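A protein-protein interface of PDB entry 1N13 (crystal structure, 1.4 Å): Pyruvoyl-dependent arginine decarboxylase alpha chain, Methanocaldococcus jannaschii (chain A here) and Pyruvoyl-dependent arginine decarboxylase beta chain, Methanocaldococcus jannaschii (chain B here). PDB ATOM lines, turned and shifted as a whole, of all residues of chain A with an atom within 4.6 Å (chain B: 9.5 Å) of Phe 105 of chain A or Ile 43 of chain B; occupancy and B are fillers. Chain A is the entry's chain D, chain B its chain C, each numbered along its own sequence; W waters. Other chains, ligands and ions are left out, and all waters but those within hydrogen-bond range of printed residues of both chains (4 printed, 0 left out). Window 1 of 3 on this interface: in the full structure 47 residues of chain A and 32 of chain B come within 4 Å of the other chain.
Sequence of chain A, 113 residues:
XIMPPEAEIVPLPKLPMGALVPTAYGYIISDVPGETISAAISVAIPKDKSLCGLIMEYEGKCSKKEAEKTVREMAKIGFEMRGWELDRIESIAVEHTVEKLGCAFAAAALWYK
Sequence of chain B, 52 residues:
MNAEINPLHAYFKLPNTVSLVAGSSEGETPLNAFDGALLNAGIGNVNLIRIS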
ATOM      1  N   LEU A  12     -13.702  16.322 -17.163  1.00  0.00           N
ATOM      2  CA  LEU A  12     -12.786  17.410 -16.828  1.00  0.00           C
ATOM      3  C   LEU A  12     -13.167  18.023 -15.486  1.00  0.00           C
ATOM      4  O   LEU A  12     -14.315  18.434 -15.286  1.00  0.00           O
ATOM      5  CB  LEU A  12     -12.813  18.490 -17.913  1.00  0.00           C
ATOM      6  CG  LEU A  12     -11.719  19.561 -17.830  1.00  0.00           C
ATOM      7  CD1 LEU A  12     -10.369  18.939 -18.179  1.00  0.00           C
ATOM      8  CD2 LEU A  12     -12.038  20.705 -18.785  1.00  0.00           C
ATOM      9  N   LEU A  15     -10.735  23.058 -12.982  1.00  0.00           N
ATOM     10  CA  LEU A  15      -9.318  23.408 -12.929  1.00  0.00           C
ATOM     11  C   LEU A  15      -9.048  24.831 -12.460  1.00  0.00           C
ATOM     12  O   LEU A  15      -9.731  25.774 -12.868  1.00  0.00           O
ATOM     13  CB  LEU A  15      -8.668  23.199 -14.301  1.00  0.00           C
ATOM     14  CG  LEU A  15      -8.604  21.775 -14.859  1.00  0.00           C
ATOM     15  CD1 LEU A  15      -8.187  21.805 -16.313  1.00  0.00           C
ATOM     16  CD2 LEU A  15      -7.642  20.928 -14.045  1.00  0.00           C
ATOM     17  N   TYR A  25      -1.672  16.438 -26.578  1.00  0.00           N
ATOM     18  CA  TYR A  25      -2.655  16.977 -27.507  1.00  0.00           C
ATOM     19  C   TYR A  25      -2.246  16.962 -28.964  1.00  0.00           C
ATOM     20  O   TYR A  25      -1.073  16.811 -29.300  1.00  0.00           O
ATOM     21  CB  TYR A  25      -3.078  18.399 -27.102  1.00  0.00           C
ATOM     22  CG  TYR A  25      -1.977  19.442 -27.121  1.00  0.00           C
ATOM     23  CD1 TYR A  25      -1.631  20.102 -28.303  1.00  0.00           C
ATOM     24  CD2 TYR A  25      -1.314  19.800 -25.952  1.00  0.00           C
ATOM     25  CE1 TYR A  25      -0.651  21.099 -28.315  1.00  0.00           C
ATOM     26  CE2 TYR A  25      -0.333  20.794 -25.951  1.00  0.00           C
ATOM     27  CZ  TYR A  25      -0.009  21.437 -27.133  1.00  0.00           C
ATOM     28  OH  TYR A  25       0.953  22.418 -27.133  1.00  0.00           O
ATOM     29  N   GLY A  26      -3.258  17.063 -29.816  1.00  0.00           N
ATOM     30  CA  GLY A  26      -3.055  17.112 -31.249  1.00  0.00           C
ATOM     31  C   GLY A  26      -3.856  18.298 -31.742  1.00  0.00           C
ATOM     32  O   GLY A  26      -4.900  18.617 -31.178  1.00  0.00           O
ATOM     33  N   TYR A  27      -3.345  19.004 -32.742  1.00  0.00           N
ATOM     34  CA  TYR A  27      -4.066  20.152 -33.271  1.00  0.00           C
ATOM     35  C   TYR A  27      -3.666  20.385 -34.717  1.00  0.00           C
ATOM     36  O   TYR A  27      -2.614  19.933 -35.165  1.00  0.00           O
ATOM     37  CB  TYR A  27      -3.793  21.417 -32.436  1.00  0.00           C
ATOM     38  CG  TYR A  27      -2.430  22.020 -32.678  1.00  0.00           C
ATOM     39  CD1 TYR A  27      -2.264  23.067 -33.588  1.00  0.00           C
ATOM     40  CD2 TYR A  27      -1.299  21.508 -32.046  1.00  0.00           C
ATOM     41  CE1 TYR A  27      -1.005  23.581 -33.869  1.00  0.00           C
ATOM     42  CE2 TYR A  27      -0.035  22.017 -32.318  1.00  0.00           C
ATOM     43  CZ  TYR A  27       0.104  23.050 -33.234  1.00  0.00           C
ATOM     44  OH  TYR A  27       1.351  23.539 -33.532  1.00  0.00           O
ATOM     45  N   ALA A  39      -9.156  16.702 -35.285  1.00  0.00           N
ATOM     46  CA  ALA A  39      -8.168  16.330 -34.287  1.00  0.00           C
ATOM     47  C   ALA A  39      -8.859  15.289 -33.409  1.00  0.00           C
ATOM     48  O   ALA A  39     -10.070  15.353 -33.192  1.00  0.00           O
ATOM     49  CB  ALA A  39      -7.751  17.536 -33.470  1.00  0.00           C
ATOM     50  N   VAL A  94     -12.997  15.841 -32.998  1.00  0.00           N
ATOM     51  CA  VAL A  94     -13.710  17.059 -33.357  1.00  0.00           C
ATOM     52  C   VAL A  94     -13.284  17.452 -34.763  1.00  0.00           C
ATOM     53  O   VAL A  94     -12.160  17.171 -35.180  1.00  0.00           O
ATOM     54  CB  VAL A  94     -13.385  18.220 -32.376  1.00  0.00           C
ATOM     55  CG1 VAL A  94     -11.901  18.585 -32.437  1.00  0.00           C
ATOM     56  CG2 VAL A  94     -14.244  19.430 -32.684  1.00  0.00           C
ATOM     57  N   CYS A 103      -8.983  26.150 -36.282  1.00  0.00           N
ATOM     58  CA  CYS A 103      -8.157  25.181 -35.576  1.00  0.00           C
ATOM     59  C   CYS A 103      -9.006  24.094 -34.936  1.00  0.00           C
ATOM     60  O   CYS A 103     -10.050  24.383 -34.355  1.00  0.00           O
ATOM     61  CB  CYS A 103      -7.345  25.880 -34.482  1.00  0.00           C
ATOM     62  SG  CYS A 103      -6.482  24.745 -33.347  1.00  0.00           S
ATOM     63  N   ALA A 104      -8.573  22.846 -35.100  1.00  0.00           N
ATOM     64  CA  ALA A 104      -9.233  21.686 -34.505  1.00  0.00           C
ATOM     65  C   ALA A 104      -8.230  21.200 -33.450  1.00  0.00           C
ATOM     66  O   ALA A 104      -7.026  21.125 -33.718  1.00  0.00           O
ATOM     67  CB  ALA A 104      -9.496  20.612 -35.550  1.00  0.00           C
ATOM     68  N   PHE A 105      -8.729  20.866 -32.264  1.00  0.00           N
ATOM     69  CA  PHE A 105      -7.881  20.474 -31.141  1.00  0.00           C
ATOM     70  C   PHE A 105      -8.497  19.359 -30.289  1.00  0.00           C
ATOM     71  O   PHE A 105      -9.692  19.372 -30.010  1.00  0.00           O
ATOM     72  CB  PHE A 105      -7.660  21.738 -30.288  1.00  0.00           C
ATOM     73  CG  PHE A 105      -7.010  21.500 -28.950  1.00  0.00           C
ATOM     74  CD1 PHE A 105      -5.627  21.532 -28.821  1.00  0.00           C
ATOM     75  CD2 PHE A 105      -7.784  21.303 -27.808  1.00  0.00           C
ATOM     76  CE1 PHE A 105      -5.022  21.376 -27.574  1.00  0.00           C
ATOM     77  CE2 PHE A 105      -7.188  21.144 -26.558  1.00  0.00           C
ATOM     78  CZ  PHE A 105      -5.803  21.182 -26.442  1.00  0.00           C
ATOM     79  N   ALA A 106      -7.663  18.405 -29.877  1.00  0.00           N
ATOM     80  CA  ALA A 106      -8.095  17.298 -29.027  1.00  0.00           C
ATOM     81  C   ALA A 106      -6.971  17.045 -28.030  1.00  0.00           C
ATOM     82  O   ALA A 106      -5.798  17.068 -28.402  1.00  0.00           O
ATOM     83  CB  ALA A 106      -8.371  16.048 -29.857  1.00  0.00           C
ATOM     84  N   ALA A 107      -7.332  16.762 -26.780  1.00  0.00           N
ATOM     85  CA  ALA A 107      -6.336  16.563 -25.742  1.00  0.00           C
ATOM     86  C   ALA A 107      -6.735  15.640 -24.602  1.00  0.00           C
ATOM     87  O   ALA A 107      -7.913  15.384 -24.362  1.00  0.00           O
ATOM     88  CB  ALA A 107      -5.950  17.926 -25.162  1.00  0.00           C
ATOM     89  N   SER B  19      -8.507  13.328 -18.451  1.00  0.00           N
ATOM     90  CA  SER B  19      -9.762  13.797 -19.024  1.00  0.00           C
ATOM     91  C   SER B  19      -9.565  14.081 -20.501  1.00  0.00           C
ATOM     92  O   SER B  19      -8.587  14.726 -20.888  1.00  0.00           O
ATOM     93  CB  SER B  19     -10.239  15.066 -18.313  1.00  0.00           C
ATOM     94  OG  SER B  19     -10.451  14.830 -16.933  1.00  0.00           O
ATOM     95  N   LEU B  20     -10.479  13.573 -21.323  1.00  0.00           N
ATOM     96  CA  LEU B  20     -10.407  13.784 -22.764  1.00  0.00           C
ATOM     97  C   LEU B  20     -11.302  14.952 -23.162  1.00  0.00           C
ATOM     98  O   LEU B  20     -12.505  14.943 -22.892  1.00  0.00           O
ATOM     99  CB  LEU B  20     -10.839  12.519 -23.519  1.00  0.00           C
ATOM    100  CG  LEU B  20     -10.029  11.250 -23.248  1.00  0.00           C
ATOM    101  CD1 LEU B  20     -10.483  10.133 -24.180  1.00  0.00           C
ATOM    102  CD2 LEU B  20      -8.550  11.532 -23.450  1.00  0.00           C
ATOM    103  N   VAL B  21     -10.709  15.951 -23.807  1.00  0.00           N
ATOM    104  CA  VAL B  21     -11.442  17.133 -24.253  1.00  0.00           C
ATOM    105  C   VAL B  21     -11.101  17.439 -25.707  1.00  0.00           C
ATOM    106  O   VAL B  21     -10.071  17.000 -26.222  1.00  0.00           O
ATOM    107  CB  VAL B  21     -11.108  18.370 -23.404  1.00  0.00           C
ATOM    108  CG1 VAL B  21     -11.530  18.150 -21.945  1.00  0.00           C
ATOM    109  CG2 VAL B  21      -9.625  18.690 -23.511  1.00  0.00           C
ATOM    110  N   ALA B  22     -11.966  18.202 -26.365  1.00  0.00           N
ATOM    111  CA  ALA B  22     -11.741  18.555 -27.757  1.00  0.00           C
ATOM    112  C   ALA B  22     -12.564  19.778 -28.104  1.00  0.00           C
ATOM    113  O   ALA B  22     -13.612  20.023 -27.504  1.00  0.00           O
ATOM    114  CB  ALA B  22     -12.113  17.385 -28.675  1.00  0.00           C
ATOM    115  N   GLY B  23     -12.074  20.553 -29.063  1.00  0.00           N
ATOM    116  CA  GLY B  23     -12.788  21.748 -29.468  1.00  0.00           C
ATOM    117  C   GLY B  23     -12.216  22.343 -30.734  1.00  0.00           C
ATOM    118  O   GLY B  23     -11.188  21.898 -31.229  1.00  0.00           O
ATOM    119  N   SER B  24     -12.917  23.322 -31.291  1.00  0.00           N
ATOM    120  CA  SER B  24     -12.451  23.975 -32.501  1.00  0.00           C
ATOM    121  C   SER B  24     -12.901  25.420 -32.464  1.00  0.00           C
ATOM    122  O   SER B  24     -13.815  25.780 -31.713  1.00  0.00           O
ATOM    123  CB  SER B  24     -12.997  23.278 -33.750  1.00  0.00           C
ATOM    124  OG  SER B  24     -14.388  23.500 -33.898  1.00  0.00           O
ATOM    125  N   SER B  25     -12.247  26.250 -33.266  1.00  0.00           N
ATOM    126  CA  SER B  25     -12.584  27.662 -33.313  1.00  0.00           C
ATOM    127  C   SER B  25     -11.913  28.362 -34.471  1.00  0.00           C
ATOM    128  O   SER B  25     -10.907  27.894 -35.008  1.00  0.00           O
ATOM    129  CB  SER B  25     -12.149  28.347 -32.010  1.00  0.00           C
ATOM    130  OG  SER B  25     -12.416  29.746 -32.019  1.00  0.00           O
ATOM    131  N   ALA B  33      -6.732  31.317 -32.919  1.00  0.00           N
ATOM    132  CA  ALA B  33      -7.617  30.208 -33.288  1.00  0.00           C
ATOM    133  C   ALA B  33      -7.352  29.036 -32.345  1.00  0.00           C
ATOM    134  O   ALA B  33      -8.280  28.358 -31.905  1.00  0.00           O
ATOM    135  CB  ALA B  33      -7.374  29.788 -34.735  1.00  0.00           C
ATOM    136  N   PHE B  34      -6.075  28.820 -32.031  1.00  0.00           N
ATOM    137  CA  PHE B  34      -5.656  27.753 -31.125  1.00  0.00           C
ATOM    138  C   PHE B  34      -6.274  28.030 -29.756  1.00  0.00           C
ATOM    139  O   PHE B  34      -6.924  27.159 -29.170  1.00  0.00           O
ATOM    140  CB  PHE B  34      -4.122  27.717 -31.041  1.00  0.00           C
ATOM    141  CG  PHE B  34      -3.575  26.637 -30.138  1.00  0.00           C
ATOM    142  CD1 PHE B  34      -3.535  25.313 -30.557  1.00  0.00           C
ATOM    143  CD2 PHE B  34      -3.082  26.954 -28.874  1.00  0.00           C
ATOM    144  CE1 PHE B  34      -3.009  24.313 -29.726  1.00  0.00           C
ATOM    145  CE2 PHE B  34      -2.557  25.966 -28.038  1.00  0.00           C
ATOM    146  CZ  PHE B  34      -2.521  24.643 -28.464  1.00  0.00           C
ATOM    147  N   ASP B  35      -6.121  29.270 -29.287  1.00  0.00           N
ATOM    148  CA  ASP B  35      -6.667  29.707 -28.004  1.00  0.00           C
ATOM    149  C   ASP B  35      -8.181  29.476 -27.996  1.00  0.00           C
ATOM    150  O   ASP B  35      -8.739  28.945 -27.035  1.00  0.00           O
ATOM    151  CB  ASP B  35      -6.349  31.199 -27.793  1.00  0.00           C
ATOM    152  CG  ASP B  35      -6.708  31.701 -26.396  1.00  0.00           C
ATOM    153  OD1 ASP B  35      -6.593  30.938 -25.414  1.00  0.00           O
ATOM    154  OD2 ASP B  35      -7.085  32.881 -26.275  1.00  0.00           O
ATOM    155  N   GLY B  36      -8.839  29.848 -29.090  1.00  0.00           N
ATOM    156  CA  GLY B  36     -10.275  29.657 -29.183  1.00  0.00           C
ATOM    157  C   GLY B  36     -10.672  28.192 -29.100  1.00  0.00           C
ATOM    158  O   GLY B  36     -11.700  27.856 -28.517  1.00  0.00           O
ATOM    159  N   ALA B  37      -9.870  27.321 -29.707  1.00  0.00           N
ATOM    160  CA  ALA B  37     -10.148  25.883 -29.695  1.00  0.00           C
ATOM    161  C   ALA B  37     -10.017  25.339 -28.276  1.00  0.00           C
ATOM    162  O   ALA B  37     -10.814  24.497 -27.843  1.00  0.00           O
ATOM    163  CB  ALA B  37      -9.204  25.149 -30.640  1.00  0.00           C
ATOM    164  N   LEU B  38      -8.987  25.795 -27.563  1.00  0.00           N
ATOM    165  CA  LEU B  38      -8.788  25.369 -26.179  1.00  0.00           C
ATOM    166  C   LEU B  38      -9.976  25.828 -25.341  1.00  0.00           C
ATOM    167  O   LEU B  38     -10.505  25.068 -24.530  1.00  0.00           O
ATOM    168  CB  LEU B  38      -7.478  25.934 -25.615  1.00  0.00           C
ATOM    169  CG  LEU B  38      -6.230  25.074 -25.827  1.00  0.00           C
ATOM    170  CD1 LEU B  38      -5.982  24.821 -27.297  1.00  0.00           C
ATOM    171  CD2 LEU B  38      -5.040  25.767 -25.196  1.00  0.00           C
ATOM    172  N   LEU B  39     -10.411  27.068 -25.558  1.00  0.00           N
ATOM    173  CA  LEU B  39     -11.561  27.609 -24.835  1.00  0.00           C
ATOM    174  C   LEU B  39     -12.804  26.773 -25.128  1.00  0.00           C
ATOM    175  O   LEU B  39     -13.576  26.450 -24.223  1.00  0.00           O
ATOM    176  CB  LEU B  39     -11.809  29.062 -25.242  1.00  0.00           C
ATOM    177  CG  LEU B  39     -10.818  30.058 -24.639  1.00  0.00           C
ATOM    178  CD1 LEU B  39     -10.901  31.386 -25.367  1.00  0.00           C
ATOM    179  CD2 LEU B  39     -11.103  30.228 -23.154  1.00  0.00           C
ATOM    180  N   ASN B  40     -12.964  26.399 -26.396  1.00  0.00           N
ATOM    181  CA  ASN B  40     -14.098  25.595 -26.846  1.00  0.00           C
ATOM    182  C   ASN B  40     -14.063  24.198 -26.222  1.00  0.00           C
ATOM    183  O   ASN B  40     -15.110  23.581 -26.008  1.00  0.00           O
ATOM    184  CB  ASN B  40     -14.084  25.499 -28.377  1.00  0.00           C
ATOM    185  CG  ASN B  40     -15.334  24.849 -28.938  1.00  0.00           C
ATOM    186  OD1 ASN B  40     -15.274  23.769 -29.524  1.00  0.00           O
ATOM    187  ND2 ASN B  40     -16.472  25.519 -28.785  1.00  0.00           N
ATOM    188  N   ALA B  41     -12.858  23.720 -25.920  1.00  0.00           N
ATOM    189  CA  ALA B  41     -12.657  22.405 -25.317  1.00  0.00           C
ATOM    190  C   ALA B  41     -12.804  22.437 -23.797  1.00  0.00           C
ATOM    191  O   ALA B  41     -12.958  21.394 -23.160  1.00  0.00           O
ATOM    192  CB  ALA B  41     -11.285  21.871 -25.691  1.00  0.00           C
ATOM    193  N   GLY B  42     -12.718  23.633 -23.219  1.00  0.00           N
ATOM    194  CA  GLY B  42     -12.850  23.777 -21.780  1.00  0.00           C
ATOM    195  C   GLY B  42     -11.550  23.922 -21.005  1.00  0.00           C
ATOM    196  O   GLY B  42     -11.574  24.017 -19.778  1.00  0.00           O
ATOM    197  N   ILE B  43     -10.410  23.965 -21.696  1.00  0.00           N
ATOM    198  CA  ILE B  43      -9.120  24.120 -21.015  1.00  0.00           C
ATOM    199  C   ILE B  43      -8.366  25.363 -21.491  1.00  0.00           C
ATOM    200  O   ILE B  43      -7.133  25.414 -21.458  1.00  0.00           O
ATOM    201  CB  ILE B  43      -8.209  22.868 -21.170  1.00  0.00           C
ATOM    202  CG1 ILE B  43      -8.035  22.490 -22.647  1.00  0.00           C
ATOM    203  CG2 ILE B  43      -8.762  21.713 -20.350  1.00  0.00           C
ATOM    204  CD1 ILE B  43      -7.040  21.364 -22.871  1.00  0.00           C
ATOM    205  N   GLY B  44      -9.123  26.387 -21.871  1.00  0.00           N
ATOM    206  CA  GLY B  44      -8.524  27.615 -22.361  1.00  0.00           C
ATOM    207  C   GLY B  44      -7.870  28.497 -21.312  1.00  0.00           C
ATOM    208  O   GLY B  44      -7.043  29.346 -21.649  1.00  0.00           O
ATOM    209  N   ASN B  45      -8.197  28.282 -20.042  1.00  0.00           N
ATOM    210  CA  ASN B  45      -7.645  29.122 -18.988  1.00  0.00           C
ATOM    211  C   ASN B  45      -6.624  28.487 -18.051  1.00  0.00           C
ATOM    212  O   ASN B  45      -6.448  28.927 -16.914  1.00  0.00           O
ATOM    213  CB  ASN B  45      -8.779  29.806 -18.222  1.00  0.00           C
ATOM    214  CG  ASN B  45      -9.589  30.733 -19.113  1.00  0.00           C
ATOM    215  OD1 ASN B  45      -9.030  31.441 -19.950  1.00  0.00           O
ATOM    216  ND2 ASN B  45     -10.908  30.706 -18.962  1.00  0.00           N
ATOM    217  N   VAL B  46      -5.974  27.432 -18.533  1.00  0.00           N
ATOM    218  CA  VAL B  46      -4.917  26.771 -17.773  1.00  0.00           C
ATOM    219  C   VAL B  46      -3.716  26.669 -18.699  1.00  0.00           C
ATOM    220  O   VAL B  46      -3.837  26.858 -19.911  1.00  0.00           O
ATOM    221  CB  VAL B  46      -5.307  25.354 -17.274  1.00  0.00           C
ATOM    222  CG1 VAL B  46      -6.471  25.428 -16.300  1.00  0.00           C
ATOM    223  CG2 VAL B  46      -5.630  24.449 -18.434  1.00  0.00           C
ATOM    224  N   ASN B  47      -2.552  26.413 -18.122  1.00  0.00           N
ATOM    225  CA  ASN B  47      -1.327  26.275 -18.894  1.00  0.00           C
ATOM    226  C   ASN B  47      -1.145  24.833 -19.316  1.00  0.00           C
ATOM    227  O   ASN B  47      -1.208  23.932 -18.483  1.00  0.00           O
ATOM    228  CB  ASN B  47      -0.127  26.714 -18.058  1.00  0.00           C
ATOM    229  CG  ASN B  47      -0.038  28.204 -17.934  1.00  0.00           C
ATOM    230  OD1 ASN B  47       0.102  28.896 -18.933  1.00  0.00           O
ATOM    231  ND2 ASN B  47      -0.163  28.717 -16.712  1.00  0.00           N
ATOM    232  N   LEU B  48      -0.960  24.607 -20.613  1.00  0.00           N
ATOM    233  CA  LEU B  48      -0.751  23.245 -21.088  1.00  0.00           C
ATOM    234  C   LEU B  48       0.741  22.937 -21.128  1.00  0.00           C
ATOM    235  O   LEU B  48       1.521  23.696 -21.697  1.00  0.00           O
ATOM    236  CB  LEU B  48      -1.340  23.046 -22.486  1.00  0.00           C
ATOM    237  CG  LEU B  48      -2.828  23.320 -22.696  1.00  0.00           C
ATOM    238  CD1 LEU B  48      -3.230  22.787 -24.069  1.00  0.00           C
ATOM    239  CD2 LEU B  48      -3.647  22.645 -21.610  1.00  0.00           C
ATOM    240  N   ILE B  49       1.138  21.869 -20.445  1.00  0.00           N
ATOM    241  CA  ILE B  49       2.531  21.426 -20.444  1.00  0.00           C
ATOM    242  C   ILE B  49       2.475  20.180 -21.319  1.00  0.00           C
ATOM    243  O   ILE B  49       2.033  19.119 -20.879  1.00  0.00           O
ATOM    244  CB  ILE B  49       3.021  21.032 -19.033  1.00  0.00           C
ATOM    245  CG1 ILE B  49       2.881  22.207 -18.059  1.00  0.00           C
ATOM    246  CG2 ILE B  49       4.469  20.553 -19.097  1.00  0.00           C
ATOM    247  CD1 ILE B  49       3.738  23.387 -18.390  1.00  0.00           C
ATOM    248  N   ARG B  50       2.905  20.311 -22.567  1.00  0.00           N
ATOM    249  CA  ARG B  50       2.840  19.190 -23.495  1.00  0.00           C
ATOM    250  C   ARG B  50       3.684  17.994 -23.087  1.00  0.00           C
ATOM    251  O   ARG B  50       4.878  18.122 -22.834  1.00  0.00           O
ATOM    252  CB  ARG B  50       3.204  19.635 -24.916  1.00  0.00           C
ATOM    253  CG  ARG B  50       2.835  18.610 -25.979  1.00  0.00           C
ATOM    254  CD  ARG B  50       2.898  19.196 -27.383  1.00  0.00           C
ATOM    255  NE  ARG B  50       2.138  18.382 -28.331  1.00  0.00           N
ATOM    256  CZ  ARG B  50       1.960  18.682 -29.615  1.00  0.00           C
ATOM    257  NH1 ARG B  50       2.487  19.788 -30.127  1.00  0.00           N
ATOM    258  NH2 ARG B  50       1.258  17.866 -30.393  1.00  0.00           N
HETATM  259  O   HOH W   1     -13.542  15.365 -20.373  1.00  0.00           O
HETATM  260  O   HOH W   2       1.118  15.910 -27.152  1.00  0.00           O
HETATM  261  O   HOH W   3       3.227  22.185 -28.878  1.00  0.00           O
HETATM  262  O   HOH W   4      -0.257  18.154 -33.082  1.00  0.00           O
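The backbone carbonyl oxygen of Tyr 25 of chain A lies within hydrogen-bond range of the guanidinium group of Arg 50 of chain B.
N of Cys 103 of chain A sits at hydrogen-bond distance from O of Ser 25 of chain B, 2.9 Å away.
O of Phe 105 of chain A lies within hydrogen-bond range of N of Gly 23 of chain B, at 2.8 Å.
O of Val 21 of chain B sits at hydrogen-bond distance from N of Ala 107 of chain A (2.8 Å).
N of Ile 43 of chain B sits at hydrogen-bond distance from O of Leu 38 of chain B, 3.0 Å away.
The backbone NH of Ser 24 of chain B sits at hydrogen-bond distance from the side-chain amide oxygen of Asn 40 of chain B (3.0 Å).
O of Ala 39 of chain A lies within hydrogen-bond range of N of Val 94 of chain A (3.0 Å).
The backbone carbonyl oxygen (O) of Ala 106 of chain A lies within hydrogen-bond range of the backbone NH (N) of Gly 26 of chain A (2.9 Å).
N of Gly 44 of chain B lies within hydrogen-bond range of O of Leu 38 of chain B.
Water W1 bridges the backbone carbonyl oxygen (O) of Leu 20 of chain B and the backbone NH (N) of Leu 12 of chain A.
Water W3 lies within hydrogen-bond range of the guanidinium group of Arg 50 of chain B (2.8 Å) and the side-chain hydroxyl of Tyr 25 of chain A (2.9 Å).
Water W2 lies within hydrogen-bond range of N of Tyr 25 of chain A and NE of Arg 50 of chain B.
Water W4 bridges NH2 of Arg 50 of chain B (3.1 Å) and N of Tyr 27 of chain A (3.2 Å).
Printed residues of chain B that touch a printed residue of chain A: Ser 19, Leu 20, Val 21, Ala 22, Gly 23, Ser 24, Ser 25, Ala 33, Phe 34, Ala 37, Leu 38, Gly 42, Ile 43, Val 46, Leu 48 and Arg 50.
Hydrophobic or aromatic side chains of chain B within 4 Å of the printed part of chain A: Val 21, Ala 22, Ala 33, Phe 34, Ala 37, Leu 38, Ile 43, Val 46 and Leu 48.
Among the printed residues, 26 pairs touch across the chains.
Among the printed residues, no Asp or Glu carboxylate lies within 4 Å of a Lys or Arg side-chain nitrogen of the other chain.
Printed residues of chain B within 4 Å of Phe 105 of chain A: Ala 22 (3.2 Å), Gly 23 (2.8 Å), Phe 34 (3.9 Å), Ala 37 (3.8 Å), Leu 38 (3.6 Å), Ile 43 (3.7 Å) and Leu 48 (3.9 Å).
Of the printed residues of chain A, Ile 43 of chain B touches Leu 12 and Phe 105.
No residue of chain B comes within 4 Å of Ala 39 of chain A.
Of the printed residues of chain A, Leu 48 of chain B touches Tyr 25 and Phe 105.
Of the printed residues of chain A, Ser 24 of chain B touches Cys 103 (3.1 Å).
Of the printed residues of chain B, Tyr 25 of chain A touches Leu 48 and Arg 50.
Of the printed residues of chain A, Arg 50 of chain B touches Tyr 25.
Asp 35 of chain B touches none of the printed residues of chain A.
Asn 45 of chain B touches none of the printed residues of chain A.
The nearest printed residue of chain A that does not touch Ile 43 of chain B is Leu 15 of chain A (4.1 Å).
The nearest printed residue of chain A that does not touch Ala 33 of chain B is Ala 104 of chain A (6.4 Å).
Among the printed residues, merely in contact across the chains: Cys 103 of chain A with Ser 24 of chain B, Phe 105 of chain A with Ala 22 of chain B, Ala 107 of chain A with Leu 20 of chain B, Ala 106 of chain A with Val 21 of chain B, Leu 12 of chain A with Ser 19 of chain B, Leu 12 of chain A with Gly 42 of chain B, Phe 105 of chain A with Leu 38 of chain B, Val 94 of chain A with Gly 23 of chain B, Ala 107 of chain A with Ser 19 of chain B, Cys 103 of chain A with Ala 33 of chain B, Phe 105 of chain A with Ile 43 of chain B, Leu 15 of chain A with Val 46 of chain B, Phe 105 of chain A with Ala 37 of chain B, Ala 104 of chain A with Gly 23 of chain B, Leu 12 of chain A with Ile 43 of chain B, Tyr 27 of chain A with Phe 34 of chain B, Cys 103 of chain A with Phe 34 of chain B, Phe 105 of chain A with Leu 48 of chain B, Cys 103 of chain A with Ala 37 of chain B, Phe 105 of chain A with Phe 34 of chain B, Val 94 of chain A with Ala 22 of chain B and Tyr 25 of chain A with Leu 48 of chain B.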
